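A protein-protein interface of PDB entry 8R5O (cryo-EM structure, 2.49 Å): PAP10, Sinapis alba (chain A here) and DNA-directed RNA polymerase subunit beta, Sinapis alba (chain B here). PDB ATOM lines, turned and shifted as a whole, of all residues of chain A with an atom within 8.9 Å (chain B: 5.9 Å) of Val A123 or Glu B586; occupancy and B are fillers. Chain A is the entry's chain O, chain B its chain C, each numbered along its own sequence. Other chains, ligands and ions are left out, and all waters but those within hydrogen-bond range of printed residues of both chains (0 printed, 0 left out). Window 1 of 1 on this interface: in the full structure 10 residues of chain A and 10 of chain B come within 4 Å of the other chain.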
ATOM      1  N   VAL A  73      32.596 -11.839 -12.113  1.00  0.00           N
ATOM      2  CA  VAL A  73      32.744 -12.909 -11.133  1.00  0.00           C
ATOM      3  C   VAL A  73      31.943 -12.529  -9.895  1.00  0.00           C
ATOM      4  O   VAL A  73      32.228 -11.511  -9.254  1.00  0.00           O
ATOM      5  CB  VAL A  73      34.217 -13.161 -10.775  1.00  0.00           C
ATOM      6  CG1 VAL A  73      34.330 -14.283  -9.756  1.00  0.00           C
ATOM      7  CG2 VAL A  73      35.020 -13.488 -12.026  1.00  0.00           C
ATOM      8  N   ARG A  74      30.944 -13.343  -9.568  1.00  0.00           N
ATOM      9  CA  ARG A  74      30.126 -13.099  -8.389  1.00  0.00           C
ATOM     10  C   ARG A  74      30.956 -13.266  -7.122  1.00  0.00           C
ATOM     11  O   ARG A  74      31.789 -14.172  -7.021  1.00  0.00           O
ATOM     12  CB  ARG A  74      28.933 -14.054  -8.380  1.00  0.00           C
ATOM     13  CG  ARG A  74      28.002 -13.914  -7.191  1.00  0.00           C
ATOM     14  CD  ARG A  74      27.358 -12.541  -7.139  1.00  0.00           C
ATOM     15  NE  ARG A  74      26.224 -12.514  -6.224  1.00  0.00           N
ATOM     16  CZ  ARG A  74      25.635 -11.410  -5.789  1.00  0.00           C
ATOM     17  NH1 ARG A  74      26.063 -10.211  -6.148  1.00  0.00           N
ATOM     18  NH2 ARG A  74      24.592 -11.511  -4.970  1.00  0.00           N
ATOM     19  N   GLU A  75      30.738 -12.381  -6.154  1.00  0.00           N
ATOM     20  CA  GLU A  75      31.477 -12.462  -4.903  1.00  0.00           C
ATOM     21  C   GLU A  75      31.047 -13.693  -4.110  1.00  0.00           C
ATOM     22  O   GLU A  75      29.906 -14.155  -4.201  1.00  0.00           O
ATOM     23  CB  GLU A  75      31.279 -11.192  -4.072  1.00  0.00           C
ATOM     24  CG  GLU A  75      30.047 -11.194  -3.186  1.00  0.00           C
ATOM     25  CD  GLU A  75      28.759 -11.053  -3.968  1.00  0.00           C
ATOM     26  OE1 GLU A  75      28.770 -10.381  -5.019  1.00  0.00           O
ATOM     27  OE2 GLU A  75      27.733 -11.614  -3.528  1.00  0.00           O
ATOM     28  N   ASP A  76      31.986 -14.234  -3.335  1.00  0.00           N
ATOM     29  CA  ASP A  76      31.766 -15.488  -2.627  1.00  0.00           C
ATOM     30  C   ASP A  76      31.069 -15.318  -1.285  1.00  0.00           C
ATOM     31  O   ASP A  76      30.637 -16.320  -0.706  1.00  0.00           O
ATOM     32  CB  ASP A  76      33.099 -16.209  -2.418  1.00  0.00           C
ATOM     33  CG  ASP A  76      33.545 -16.979  -3.644  1.00  0.00           C
ATOM     34  OD1 ASP A  76      32.712 -17.708  -4.220  1.00  0.00           O
ATOM     35  OD2 ASP A  76      34.726 -16.857  -4.032  1.00  0.00           O
ATOM     36  N   TYR A  77      30.941 -14.095  -0.776  1.00  0.00           N
ATOM     37  CA  TYR A  77      30.404 -13.880   0.561  1.00  0.00           C
ATOM     38  C   TYR A  77      29.429 -12.716   0.554  1.00  0.00           C
ATOM     39  O   TYR A  77      29.741 -11.639   0.037  1.00  0.00           O
ATOM     40  CB  TYR A  77      31.534 -13.631   1.567  1.00  0.00           C
ATOM     41  CG  TYR A  77      32.457 -14.815   1.707  1.00  0.00           C
ATOM     42  CD1 TYR A  77      32.118 -15.889   2.519  1.00  0.00           C
ATOM     43  CD2 TYR A  77      33.659 -14.871   1.016  1.00  0.00           C
ATOM     44  CE1 TYR A  77      32.952 -16.980   2.645  1.00  0.00           C
ATOM     45  CE2 TYR A  77      34.501 -15.957   1.137  1.00  0.00           C
ATOM     46  CZ  TYR A  77      34.141 -17.010   1.952  1.00  0.00           C
ATOM     47  OH  TYR A  77      34.975 -18.095   2.078  1.00  0.00           O
ATOM     48  N   LEU A  78      28.253 -12.934   1.142  1.00  0.00           N
ATOM     49  CA  LEU A  78      27.186 -11.942   1.143  1.00  0.00           C
ATOM     50  C   LEU A  78      27.159 -11.088   2.404  1.00  0.00           C
ATOM     51  O   LEU A  78      26.744  -9.926   2.342  1.00  0.00           O
ATOM     52  CB  LEU A  78      25.827 -12.628   0.972  1.00  0.00           C
ATOM     53  CG  LEU A  78      25.302 -12.905  -0.443  1.00  0.00           C
ATOM     54  CD1 LEU A  78      26.298 -13.692  -1.276  1.00  0.00           C
ATOM     55  CD2 LEU A  78      23.976 -13.644  -0.369  1.00  0.00           C
ATOM     56  N   VAL A  79      27.584 -11.629   3.541  1.00  0.00           N
ATOM     57  CA  VAL A  79      27.498 -10.908   4.808  1.00  0.00           C
ATOM     58  C   VAL A  79      28.624  -9.884   4.871  1.00  0.00           C
ATOM     59  O   VAL A  79      29.801 -10.228   4.713  1.00  0.00           O
ATOM     60  CB  VAL A  79      27.558 -11.873   6.000  1.00  0.00           C
ATOM     61  CG1 VAL A  79      27.516 -11.101   7.309  1.00  0.00           C
ATOM     62  CG2 VAL A  79      26.416 -12.871   5.930  1.00  0.00           C
ATOM     63  N   GLN A 116      28.833 -19.940   8.421  1.00  0.00           N
ATOM     64  CA  GLN A 116      28.199 -20.653   7.319  1.00  0.00           C
ATOM     65  C   GLN A 116      26.679 -20.576   7.387  1.00  0.00           C
ATOM     66  O   GLN A 116      26.015 -20.568   6.346  1.00  0.00           O
ATOM     67  CB  GLN A 116      28.657 -22.109   7.303  1.00  0.00           C
ATOM     68  CG  GLN A 116      30.137 -22.287   7.028  1.00  0.00           C
ATOM     69  CD  GLN A 116      30.577 -23.730   7.136  1.00  0.00           C
ATOM     70  OE1 GLN A 116      30.612 -24.455   6.143  1.00  0.00           O
ATOM     71  NE2 GLN A 116      30.918 -24.154   8.346  1.00  0.00           N
ATOM     72  N   GLU A 117      26.109 -20.526   8.594  1.00  0.00           N
ATOM     73  CA  GLU A 117      24.658 -20.438   8.720  1.00  0.00           C
ATOM     74  C   GLU A 117      24.145 -19.069   8.291  1.00  0.00           C
ATOM     75  O   GLU A 117      23.072 -18.963   7.688  1.00  0.00           O
ATOM     76  CB  GLU A 117      24.231 -20.743  10.155  1.00  0.00           C
ATOM     77  CG  GLU A 117      24.793 -22.040  10.713  1.00  0.00           C
ATOM     78  CD  GLU A 117      24.507 -23.237   9.826  1.00  0.00           C
ATOM     79  OE1 GLU A 117      23.375 -23.346   9.308  1.00  0.00           O
ATOM     80  OE2 GLU A 117      25.420 -24.071   9.644  1.00  0.00           O
ATOM     81  N   LEU A 118      24.896 -18.008   8.596  1.00  0.00           N
ATOM     82  CA  LEU A 118      24.453 -16.665   8.238  1.00  0.00           C
ATOM     83  C   LEU A 118      24.587 -16.402   6.745  1.00  0.00           C
ATOM     84  O   LEU A 118      23.795 -15.641   6.180  1.00  0.00           O
ATOM     85  CB  LEU A 118      25.237 -15.630   9.037  1.00  0.00           C
ATOM     86  CG  LEU A 118      24.988 -15.685  10.543  1.00  0.00           C
ATOM     87  CD1 LEU A 118      26.043 -14.895  11.279  1.00  0.00           C
ATOM     88  CD2 LEU A 118      23.596 -15.166  10.875  1.00  0.00           C
ATOM     89  N   GLU A 119      25.580 -17.010   6.090  1.00  0.00           N
ATOM     90  CA  GLU A 119      25.668 -16.910   4.637  1.00  0.00           C
ATOM     91  C   GLU A 119      24.471 -17.576   3.975  1.00  0.00           C
ATOM     92  O   GLU A 119      23.933 -17.066   2.986  1.00  0.00           O
ATOM     93  CB  GLU A 119      26.975 -17.526   4.140  1.00  0.00           C
ATOM     94  CG  GLU A 119      28.216 -16.703   4.451  1.00  0.00           C
ATOM     95  CD  GLU A 119      28.287 -15.415   3.650  1.00  0.00           C
ATOM     96  OE1 GLU A 119      27.602 -15.312   2.612  1.00  0.00           O
ATOM     97  OE2 GLU A 119      29.035 -14.502   4.060  1.00  0.00           O
ATOM     98  N   MET A 120      24.039 -18.723   4.506  1.00  0.00           N
ATOM     99  CA  MET A 120      22.830 -19.365   4.003  1.00  0.00           C
ATOM    100  C   MET A 120      21.597 -18.514   4.282  1.00  0.00           C
ATOM    101  O   MET A 120      20.697 -18.421   3.440  1.00  0.00           O
ATOM    102  CB  MET A 120      22.681 -20.757   4.620  1.00  0.00           C
ATOM    103  CG  MET A 120      21.363 -21.443   4.307  1.00  0.00           C
ATOM    104  SD  MET A 120      21.032 -21.572   2.539  1.00  0.00           S
ATOM    105  CE  MET A 120      22.439 -22.530   1.993  1.00  0.00           C
ATOM    106  N   LEU A 121      21.537 -17.889   5.460  1.00  0.00           N
ATOM    107  CA  LEU A 121      20.413 -17.013   5.779  1.00  0.00           C
ATOM    108  C   LEU A 121      20.360 -15.811   4.847  1.00  0.00           C
ATOM    109  O   LEU A 121      19.272 -15.327   4.517  1.00  0.00           O
ATOM    110  CB  LEU A 121      20.504 -16.555   7.234  1.00  0.00           C
ATOM    111  CG  LEU A 121      19.246 -15.925   7.831  1.00  0.00           C
ATOM    112  CD1 LEU A 121      18.169 -16.979   8.023  1.00  0.00           C
ATOM    113  CD2 LEU A 121      19.559 -15.229   9.143  1.00  0.00           C
ATOM    114  N   ALA A 122      21.523 -15.312   4.418  1.00  0.00           N
ATOM    115  CA  ALA A 122      21.550 -14.196   3.478  1.00  0.00           C
ATOM    116  C   ALA A 122      21.022 -14.611   2.111  1.00  0.00           C
ATOM    117  O   ALA A 122      20.384 -13.811   1.418  1.00  0.00           O
ATOM    118  CB  ALA A 122      22.969 -13.643   3.364  1.00  0.00           C
ATOM    119  N   VAL A 123      21.290 -15.851   1.698  1.00  0.00           N
ATOM    120  CA  VAL A 123      20.772 -16.337   0.423  1.00  0.00           C
ATOM    121  C   VAL A 123      19.254 -16.457   0.474  1.00  0.00           C
ATOM    122  O   VAL A 123      18.558 -16.077  -0.474  1.00  0.00           O
ATOM    123  CB  VAL A 123      21.438 -17.672   0.048  1.00  0.00           C
ATOM    124  CG1 VAL A 123      20.818 -18.241  -1.217  1.00  0.00           C
ATOM    125  CG2 VAL A 123      22.934 -17.489  -0.128  1.00  0.00           C
ATOM    126  N   GLU A 124      18.716 -16.987   1.577  1.00  0.00           N
ATOM    127  CA  GLU A 124      17.268 -17.133   1.697  1.00  0.00           C
ATOM    128  C   GLU A 124      16.572 -15.778   1.718  1.00  0.00           C
ATOM    129  O   GLU A 124      15.548 -15.591   1.051  1.00  0.00           O
ATOM    130  CB  GLU A 124      16.919 -17.925   2.955  1.00  0.00           C
ATOM    131  CG  GLU A 124      17.534 -19.308   3.019  1.00  0.00           C
ATOM    132  CD  GLU A 124      16.794 -20.226   3.970  1.00  0.00           C
ATOM    133  OE1 GLU A 124      15.656 -19.888   4.358  1.00  0.00           O
ATOM    134  OE2 GLU A 124      17.349 -21.287   4.328  1.00  0.00           O
ATOM    135  N   TYR A 125      17.106 -14.825   2.479  1.00  0.00           N
ATOM    136  CA  TYR A 125      16.538 -13.481   2.569  1.00  0.00           C
ATOM    137  C   TYR A 125      17.398 -12.549   1.723  1.00  0.00           C
ATOM    138  O   TYR A 125      18.320 -11.891   2.206  1.00  0.00           O
ATOM    139  CB  TYR A 125      16.458 -13.027   4.024  1.00  0.00           C
ATOM    140  CG  TYR A 125      15.533 -13.867   4.876  1.00  0.00           C
ATOM    141  CD1 TYR A 125      15.984 -15.026   5.491  1.00  0.00           C
ATOM    142  CD2 TYR A 125      14.208 -13.500   5.065  1.00  0.00           C
ATOM    143  CE1 TYR A 125      15.142 -15.796   6.267  1.00  0.00           C
ATOM    144  CE2 TYR A 125      13.359 -14.263   5.840  1.00  0.00           C
ATOM    145  CZ  TYR A 125      13.831 -15.410   6.440  1.00  0.00           C
ATOM    146  OH  TYR A 125      12.990 -16.175   7.214  1.00  0.00           O
ATOM    147  N   GLU A 126      17.088 -12.508   0.428  1.00  0.00           N
ATOM    148  CA  GLU A 126      17.872 -11.731  -0.526  1.00  0.00           C
ATOM    149  C   GLU A 126      17.837 -10.245  -0.189  1.00  0.00           C
ATOM    150  O   GLU A 126      18.868  -9.654   0.151  1.00  0.00           O
ATOM    151  CB  GLU A 126      17.353 -11.956  -1.947  1.00  0.00           C
ATOM    152  CG  GLU A 126      17.095 -13.411  -2.289  1.00  0.00           C
ATOM    153  CD  GLU A 126      16.605 -13.593  -3.712  1.00  0.00           C
ATOM    154  OE1 GLU A 126      16.823 -12.681  -4.537  1.00  0.00           O
ATOM    155  OE2 GLU A 126      15.999 -14.646  -4.005  1.00  0.00           O
ATOM    156  N   SER A 127      16.656  -9.637  -0.274  1.00  0.00           N
ATOM    157  CA  SER A 127      16.474  -8.240   0.085  1.00  0.00           C
ATOM    158  C   SER A 127      15.442  -8.048   1.182  1.00  0.00           C
ATOM    159  O   SER A 127      15.138  -6.904   1.534  1.00  0.00           O
ATOM    160  CB  SER A 127      16.075  -7.415  -1.145  1.00  0.00           C
ATOM    161  OG  SER A 127      17.147  -7.325  -2.066  1.00  0.00           O
ATOM    162  N   ASN A 128      14.892  -9.131   1.729  1.00  0.00           N
ATOM    163  CA  ASN A 128      13.929  -9.043   2.815  1.00  0.00           C
ATOM    164  C   ASN A 128      14.594  -8.920   4.178  1.00  0.00           C
ATOM    165  O   ASN A 128      13.889  -8.780   5.182  1.00  0.00           O
ATOM    166  CB  ASN A 128      13.007 -10.262   2.791  1.00  0.00           C
ATOM    167  CG  ASN A 128      12.474 -10.562   1.404  1.00  0.00           C
ATOM    168  OD1 ASN A 128      12.991 -10.059   0.406  1.00  0.00           O
ATOM    169  ND2 ASN A 128      11.440 -11.391   1.333  1.00  0.00           N
ATOM    170  N   ALA A 129      15.922  -8.974   4.236  1.00  0.00           N
ATOM    171  CA  ALA A 129      16.655  -8.797   5.480  1.00  0.00           C
ATOM    172  C   ALA A 129      18.059  -8.320   5.148  1.00  0.00           C
ATOM    173  O   ALA A 129      18.544  -8.491   4.028  1.00  0.00           O
ATOM    174  CB  ALA A 129      16.703 -10.091   6.299  1.00  0.00           C
ATOM    175  N   ILE A 131      21.922  -8.667   6.653  1.00  0.00           N
ATOM    176  CA  ILE A 131      22.792  -9.425   7.546  1.00  0.00           C
ATOM    177  C   ILE A 131      24.157  -8.753   7.552  1.00  0.00           C
ATOM    178  O   ILE A 131      24.782  -8.593   6.495  1.00  0.00           O
ATOM    179  CB  ILE A 131      22.910 -10.894   7.113  1.00  0.00           C
ATOM    180  CG1 ILE A 131      21.542 -11.456   6.720  1.00  0.00           C
ATOM    181  CG2 ILE A 131      23.531 -11.729   8.223  1.00  0.00           C
ATOM    182  CD1 ILE A 131      20.550 -11.509   7.850  1.00  0.00           C
ATOM    183  N   LEU A 174      19.120 -22.747  12.157  1.00  0.00           N
ATOM    184  CA  LEU A 174      18.726 -21.846  11.079  1.00  0.00           C
ATOM    185  C   LEU A 174      17.225 -21.579  11.100  1.00  0.00           C
ATOM    186  O   LEU A 174      16.787 -20.447  10.868  1.00  0.00           O
ATOM    187  CB  LEU A 174      19.150 -22.431   9.732  1.00  0.00           C
ATOM    188  CG  LEU A 174      18.956 -21.564   8.488  1.00  0.00           C
ATOM    189  CD1 LEU A 174      19.828 -20.322   8.552  1.00  0.00           C
ATOM    190  CD2 LEU A 174      19.256 -22.368   7.232  1.00  0.00           C
ATOM    191  N   ALA B 583      27.342 -24.378  -8.726  1.00  0.00           N
ATOM    192  CA  ALA B 583      26.749 -23.070  -8.961  1.00  0.00           C
ATOM    193  C   ALA B 583      27.822 -21.993  -9.041  1.00  0.00           C
ATOM    194  O   ALA B 583      28.715 -21.920  -8.193  1.00  0.00           O
ATOM    195  CB  ALA B 583      25.752 -22.740  -7.852  1.00  0.00           C
ATOM    196  N   GLU B 584      27.728 -21.153 -10.067  1.00  0.00           N
ATOM    197  CA  GLU B 584      28.576 -19.978 -10.191  1.00  0.00           C
ATOM    198  C   GLU B 584      27.975 -18.762  -9.502  1.00  0.00           C
ATOM    199  O   GLU B 584      28.626 -17.715  -9.440  1.00  0.00           O
ATOM    200  CB  GLU B 584      28.835 -19.655 -11.667  1.00  0.00           C
ATOM    201  CG  GLU B 584      29.164 -20.863 -12.531  1.00  0.00           C
ATOM    202  CD  GLU B 584      27.924 -21.544 -13.081  1.00  0.00           C
ATOM    203  OE1 GLU B 584      26.815 -21.004 -12.888  1.00  0.00           O
ATOM    204  OE2 GLU B 584      28.056 -22.618 -13.704  1.00  0.00           O
ATOM    205  N   HIS B 585      26.757 -18.886  -8.983  1.00  0.00           N
ATOM    206  CA  HIS B 585      26.035 -17.780  -8.379  1.00  0.00           C
ATOM    207  C   HIS B 585      25.093 -18.345  -7.327  1.00  0.00           C
ATOM    208  O   HIS B 585      24.547 -19.439  -7.492  1.00  0.00           O
ATOM    209  CB  HIS B 585      25.258 -16.992  -9.442  1.00  0.00           C
ATOM    210  CG  HIS B 585      24.775 -15.653  -8.982  1.00  0.00           C
ATOM    211  ND1 HIS B 585      23.588 -15.484  -8.302  1.00  0.00           N
ATOM    212  CD2 HIS B 585      25.308 -14.417  -9.121  1.00  0.00           C
ATOM    213  CE1 HIS B 585      23.417 -14.201  -8.033  1.00  0.00           C
ATOM    214  NE2 HIS B 585      24.447 -13.532  -8.518  1.00  0.00           N
ATOM    215  N   GLU B 586      24.913 -17.603  -6.240  1.00  0.00           N
ATOM    216  CA  GLU B 586      23.966 -18.028  -5.220  1.00  0.00           C
ATOM    217  C   GLU B 586      22.536 -17.737  -5.673  1.00  0.00           C
ATOM    218  O   GLU B 586      22.296 -16.992  -6.626  1.00  0.00           O
ATOM    219  CB  GLU B 586      24.259 -17.340  -3.889  1.00  0.00           C
ATOM    220  CG  GLU B 586      23.725 -15.921  -3.780  1.00  0.00           C
ATOM    221  CD  GLU B 586      24.533 -14.922  -4.584  1.00  0.00           C
ATOM    222  OE1 GLU B 586      25.703 -15.218  -4.903  1.00  0.00           O
ATOM    223  OE2 GLU B 586      23.997 -13.839  -4.895  1.00  0.00           O
ATOM    224  N   GLY B 587      21.581 -18.335  -4.984  1.00  0.00           N
ATOM    225  CA  GLY B 587      20.182 -18.093  -5.285  1.00  0.00           C
ATOM    226  C   GLY B 587      19.332 -19.298  -4.917  1.00  0.00           C
ATOM    227  O   GLY B 587      19.682 -20.069  -4.027  1.00  0.00           O
ATOM    228  N   LYS B 588      18.209 -19.431  -5.624  1.00  0.00           N
ATOM    229  CA  LYS B 588      17.238 -20.490  -5.392  1.00  0.00           C
ATOM    230  C   LYS B 588      17.013 -21.279  -6.673  1.00  0.00           C
ATOM    231  O   LYS B 588      17.135 -20.746  -7.780  1.00  0.00           O
ATOM    232  CB  LYS B 588      15.893 -19.931  -4.913  1.00  0.00           C
ATOM    233  CG  LYS B 588      15.962 -18.568  -4.251  1.00  0.00           C
ATOM    234  CD  LYS B 588      16.534 -18.649  -2.853  1.00  0.00           C
ATOM    235  CE  LYS B 588      16.263 -17.371  -2.081  1.00  0.00           C
ATOM    236  NZ  LYS B 588      14.804 -17.112  -1.936  1.00  0.00           N
ATOM    237  N   LEU B 599      18.319 -21.630 -12.051  1.00  0.00           N
ATOM    238  CA  LEU B 599      18.684 -21.037 -10.774  1.00  0.00           C
ATOM    239  C   LEU B 599      18.557 -19.526 -10.882  1.00  0.00           C
ATOM    240  O   LEU B 599      19.054 -18.928 -11.840  1.00  0.00           O
ATOM    241  CB  LEU B 599      20.112 -21.428 -10.379  1.00  0.00           C
ATOM    242  CG  LEU B 599      20.802 -20.625  -9.275  1.00  0.00           C
ATOM    243  CD1 LEU B 599      20.340 -21.068  -7.896  1.00  0.00           C
ATOM    244  CD2 LEU B 599      22.313 -20.745  -9.404  1.00  0.00           C
ATOM    245  N   SER B 600      17.893 -18.914  -9.905  1.00  0.00           N
ATOM    246  CA  SER B 600      17.681 -17.473  -9.897  1.00  0.00           C
ATOM    247  C   SER B 600      18.137 -16.903  -8.564  1.00  0.00           C
ATOM    248  O   SER B 600      17.773 -17.422  -7.505  1.00  0.00           O
ATOM    249  CB  SER B 600      16.210 -17.125 -10.144  1.00  0.00           C
ATOM    250  OG  SER B 600      15.394 -17.579  -9.080  1.00  0.00           O
ATOM    251  N   GLY B 601      18.925 -15.834  -8.623  1.00  0.00           N
ATOM    252  CA  GLY B 601      19.381 -15.160  -7.425  1.00  0.00           C
ATOM    253  C   GLY B 601      19.733 -13.709  -7.674  1.00  0.00           C
ATOM    254  O   GLY B 601      20.486 -13.400  -8.603  1.00  0.00           O
ATOM    255  N   ASN B 602      19.188 -12.814  -6.849  1.00  0.00           N
ATOM    256  CA  ASN B 602      19.427 -11.374  -6.948  1.00  0.00           C
ATOM    257  C   ASN B 602      19.064 -10.849  -8.340  1.00  0.00           C
ATOM    258  O   ASN B 602      19.880 -10.249  -9.045  1.00  0.00           O
ATOM    259  CB  ASN B 602      20.876 -11.030  -6.584  1.00  0.00           C
ATOM    260  CG  ASN B 602      21.077  -9.550  -6.327  1.00  0.00           C
ATOM    261  OD1 ASN B 602      20.147  -8.847  -5.931  1.00  0.00           O
ATOM    262  ND2 ASN B 602      22.292  -9.067  -6.555  1.00  0.00           N
ATOM    263  N   CYS B 633      17.834 -23.439  -1.632  1.00  0.00           N
ATOM    264  CA  CYS B 633      18.789 -22.341  -1.668  1.00  0.00           C
ATOM    265  C   CYS B 633      20.202 -22.866  -1.875  1.00  0.00           C
ATOM    266  O   CYS B 633      20.589 -23.894  -1.311  1.00  0.00           O
ATOM    267  CB  CYS B 633      18.714 -21.529  -0.377  1.00  0.00           C
ATOM    268  SG  CYS B 633      17.097 -20.789  -0.077  1.00  0.00           S
ATOM    269  N   ILE B 634      20.973 -22.154  -2.691  1.00  0.00           N
ATOM    270  CA  ILE B 634      22.315 -22.568  -3.076  1.00  0.00           C
ATOM    271  C   ILE B 634      23.281 -21.430  -2.790  1.00  0.00           C
ATOM    272  O   ILE B 634      22.960 -20.258  -3.015  1.00  0.00           O
ATOM    273  CB  ILE B 634      22.385 -22.964  -4.567  1.00  0.00           C
ATOM    274  CG1 ILE B 634      21.194 -23.838  -4.958  1.00  0.00           C
ATOM    275  CG2 ILE B 634      23.680 -23.694  -4.865  1.00  0.00           C
ATOM    276  CD1 ILE B 634      21.207 -25.204  -4.326  1.00  0.00           C
ATOM    277  N   LYS B 635      24.460 -21.773  -2.283  1.00  0.00           N
ATOM    278  CA  LYS B 635      25.578 -20.845  -2.240  1.00  0.00           C
ATOM    279  C   LYS B 635      26.406 -20.977  -3.511  1.00  0.00           C
ATOM    280  O   LYS B 635      26.356 -21.992  -4.210  1.00  0.00           O
ATOM    281  CB  LYS B 635      26.467 -21.105  -1.024  1.00  0.00           C
ATOM    282  CG  LYS B 635      25.812 -20.879   0.322  1.00  0.00           C
ATOM    283  CD  LYS B 635      26.810 -21.158   1.433  1.00  0.00           C
ATOM    284  CE  LYS B 635      26.192 -20.997   2.805  1.00  0.00           C
ATOM    285  NZ  LYS B 635      27.161 -21.366   3.871  1.00  0.00           N
ATOM    286  N   LYS B 636      27.170 -19.933  -3.813  1.00  0.00           N
ATOM    287  CA  LYS B 636      28.105 -20.012  -4.925  1.00  0.00           C
ATOM    288  C   LYS B 636      29.169 -21.063  -4.632  1.00  0.00           C
ATOM    289  O   LYS B 636      29.779 -21.065  -3.561  1.00  0.00           O
ATOM    290  CB  LYS B 636      28.757 -18.655  -5.178  1.00  0.00           C
ATOM    291  CG  LYS B 636      29.917 -18.714  -6.155  1.00  0.00           C
ATOM    292  CD  LYS B 636      30.534 -17.351  -6.386  1.00  0.00           C
ATOM    293  CE  LYS B 636      31.801 -17.459  -7.214  1.00  0.00           C
ATOM    294  NZ  LYS B 636      31.548 -18.101  -8.529  1.00  0.00           N
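Among the printed residues, pairs that only touch across the chains: Arg A74 with Glu B584 (3.8 Å), Arg A74 with Asn B602 (3.7 Å), Arg A74 with Lys B636 (3.3 Å), Glu A75 with Lys B636 (3.9 Å), Asp A76 with Lys B636 (3.1 Å), Leu A78 with Glu B586 (3.9 Å), Glu A119 with Lys B635 (3.8 Å), Met A120 with Cys B633 (3.7 Å), Met A120 with Lys B635 (3.6 Å), Val A123 with Glu B586 (3.99 Å), Val A123 with Gly B587 (3.5 Å), Val A123 with Lys B588 (3.1 Å), Val A123 with Cys B633 (3.99 Å), Val A123 with Ile B634 (3.4 Å) and Glu A124 with Cys B633 (3.5 Å).
NE of Arg A74 lies within hydrogen-bond range of NE2 of His B585 (3.1 Å).
The side-chain carboxylate (OE2) of Glu A126 lies within salt-bridge range of the side-chain amino group (NZ) of Lys B588 (3.4 Å).
NH2 of Arg A74 lies within salt-bridge range of OE2 of Glu B586.
OE1 of Glu A126 sits at hydrogen-bond distance from N of Asn B602 (3.3 Å).
The backbone carbonyl oxygen (O) of Gln A116 sits at hydrogen-bond distance from the side-chain amino group (NZ) of Lys B635, at 2.8 Å.
The side-chain amino group (NZ) of Lys B588 sits at hydrogen-bond distance from the backbone carbonyl oxygen (O) of Glu A124 (3.4 Å).
Of the printed residues of chain B, Glu A75 touches Lys B636 (3.9 Å).
Printed residues of chain B within 4 Å of Val A123: Glu B586 (3.99 Å), Gly B587 (3.5 Å), Lys B588 (3.1 Å), Cys B633 (3.99 Å) and Ile B634 (3.4 Å).
Printed residues of chain B within 4 Å of Glu A126: Lys B588 (3.3 Å) and Asn B602 (3.3 Å).
Printed residues of chain A within 4 Å of Glu B586: Arg A74, Leu A78 and Val A123.
No residue of chain A comes within 4 Å of Gly B601.
The nearest printed residue of chain B that does not touch Val A123 is Lys B635 (4.5 Å).
The nearest printed residue of chain A that does not touch Glu B586 is Glu A75 (4.4 Å).
The nearest printed residue of chain B that does not touch Glu A119 is Glu B586 (6.9 Å).
Of the 23 printed residues of chain A, 10 touch a printed residue of chain B.
Of the 14 printed residues of chain B, 10 touch a printed residue of chain A.
Hydrophobic or aromatic side chains of chain B within 4 Å of the printed part of chain A: His B585.
Among the printed residues, 21 pairs touch across the chains.
The backbone carbonyl oxygen (O) of Glu B584 sits at hydrogen-bond distance from the side-chain amino group (NZ) of Lys B636 (3.1 Å).
The backbone NH (N) of Lys B588 is in hydrogen-bond range of the backbone carbonyl oxygen (O) of Ser B600 (2.8 Å).
The backbone carbonyl oxygen (O) of Gly B587 is in hydrogen-bond range of the backbone NH (N) of Ile B634 (2.8 Å).
The backbone NH of Leu A78 is in hydrogen-bond range of the side-chain carboxylate of Glu A119 (2.9 Å).
N of Val A79 is in hydrogen-bond range of OE2 of Glu A119, at 3.3 Å.
NH1 of Arg A74 lies within salt-bridge range of OE1 of Glu A75 (2.9 Å).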
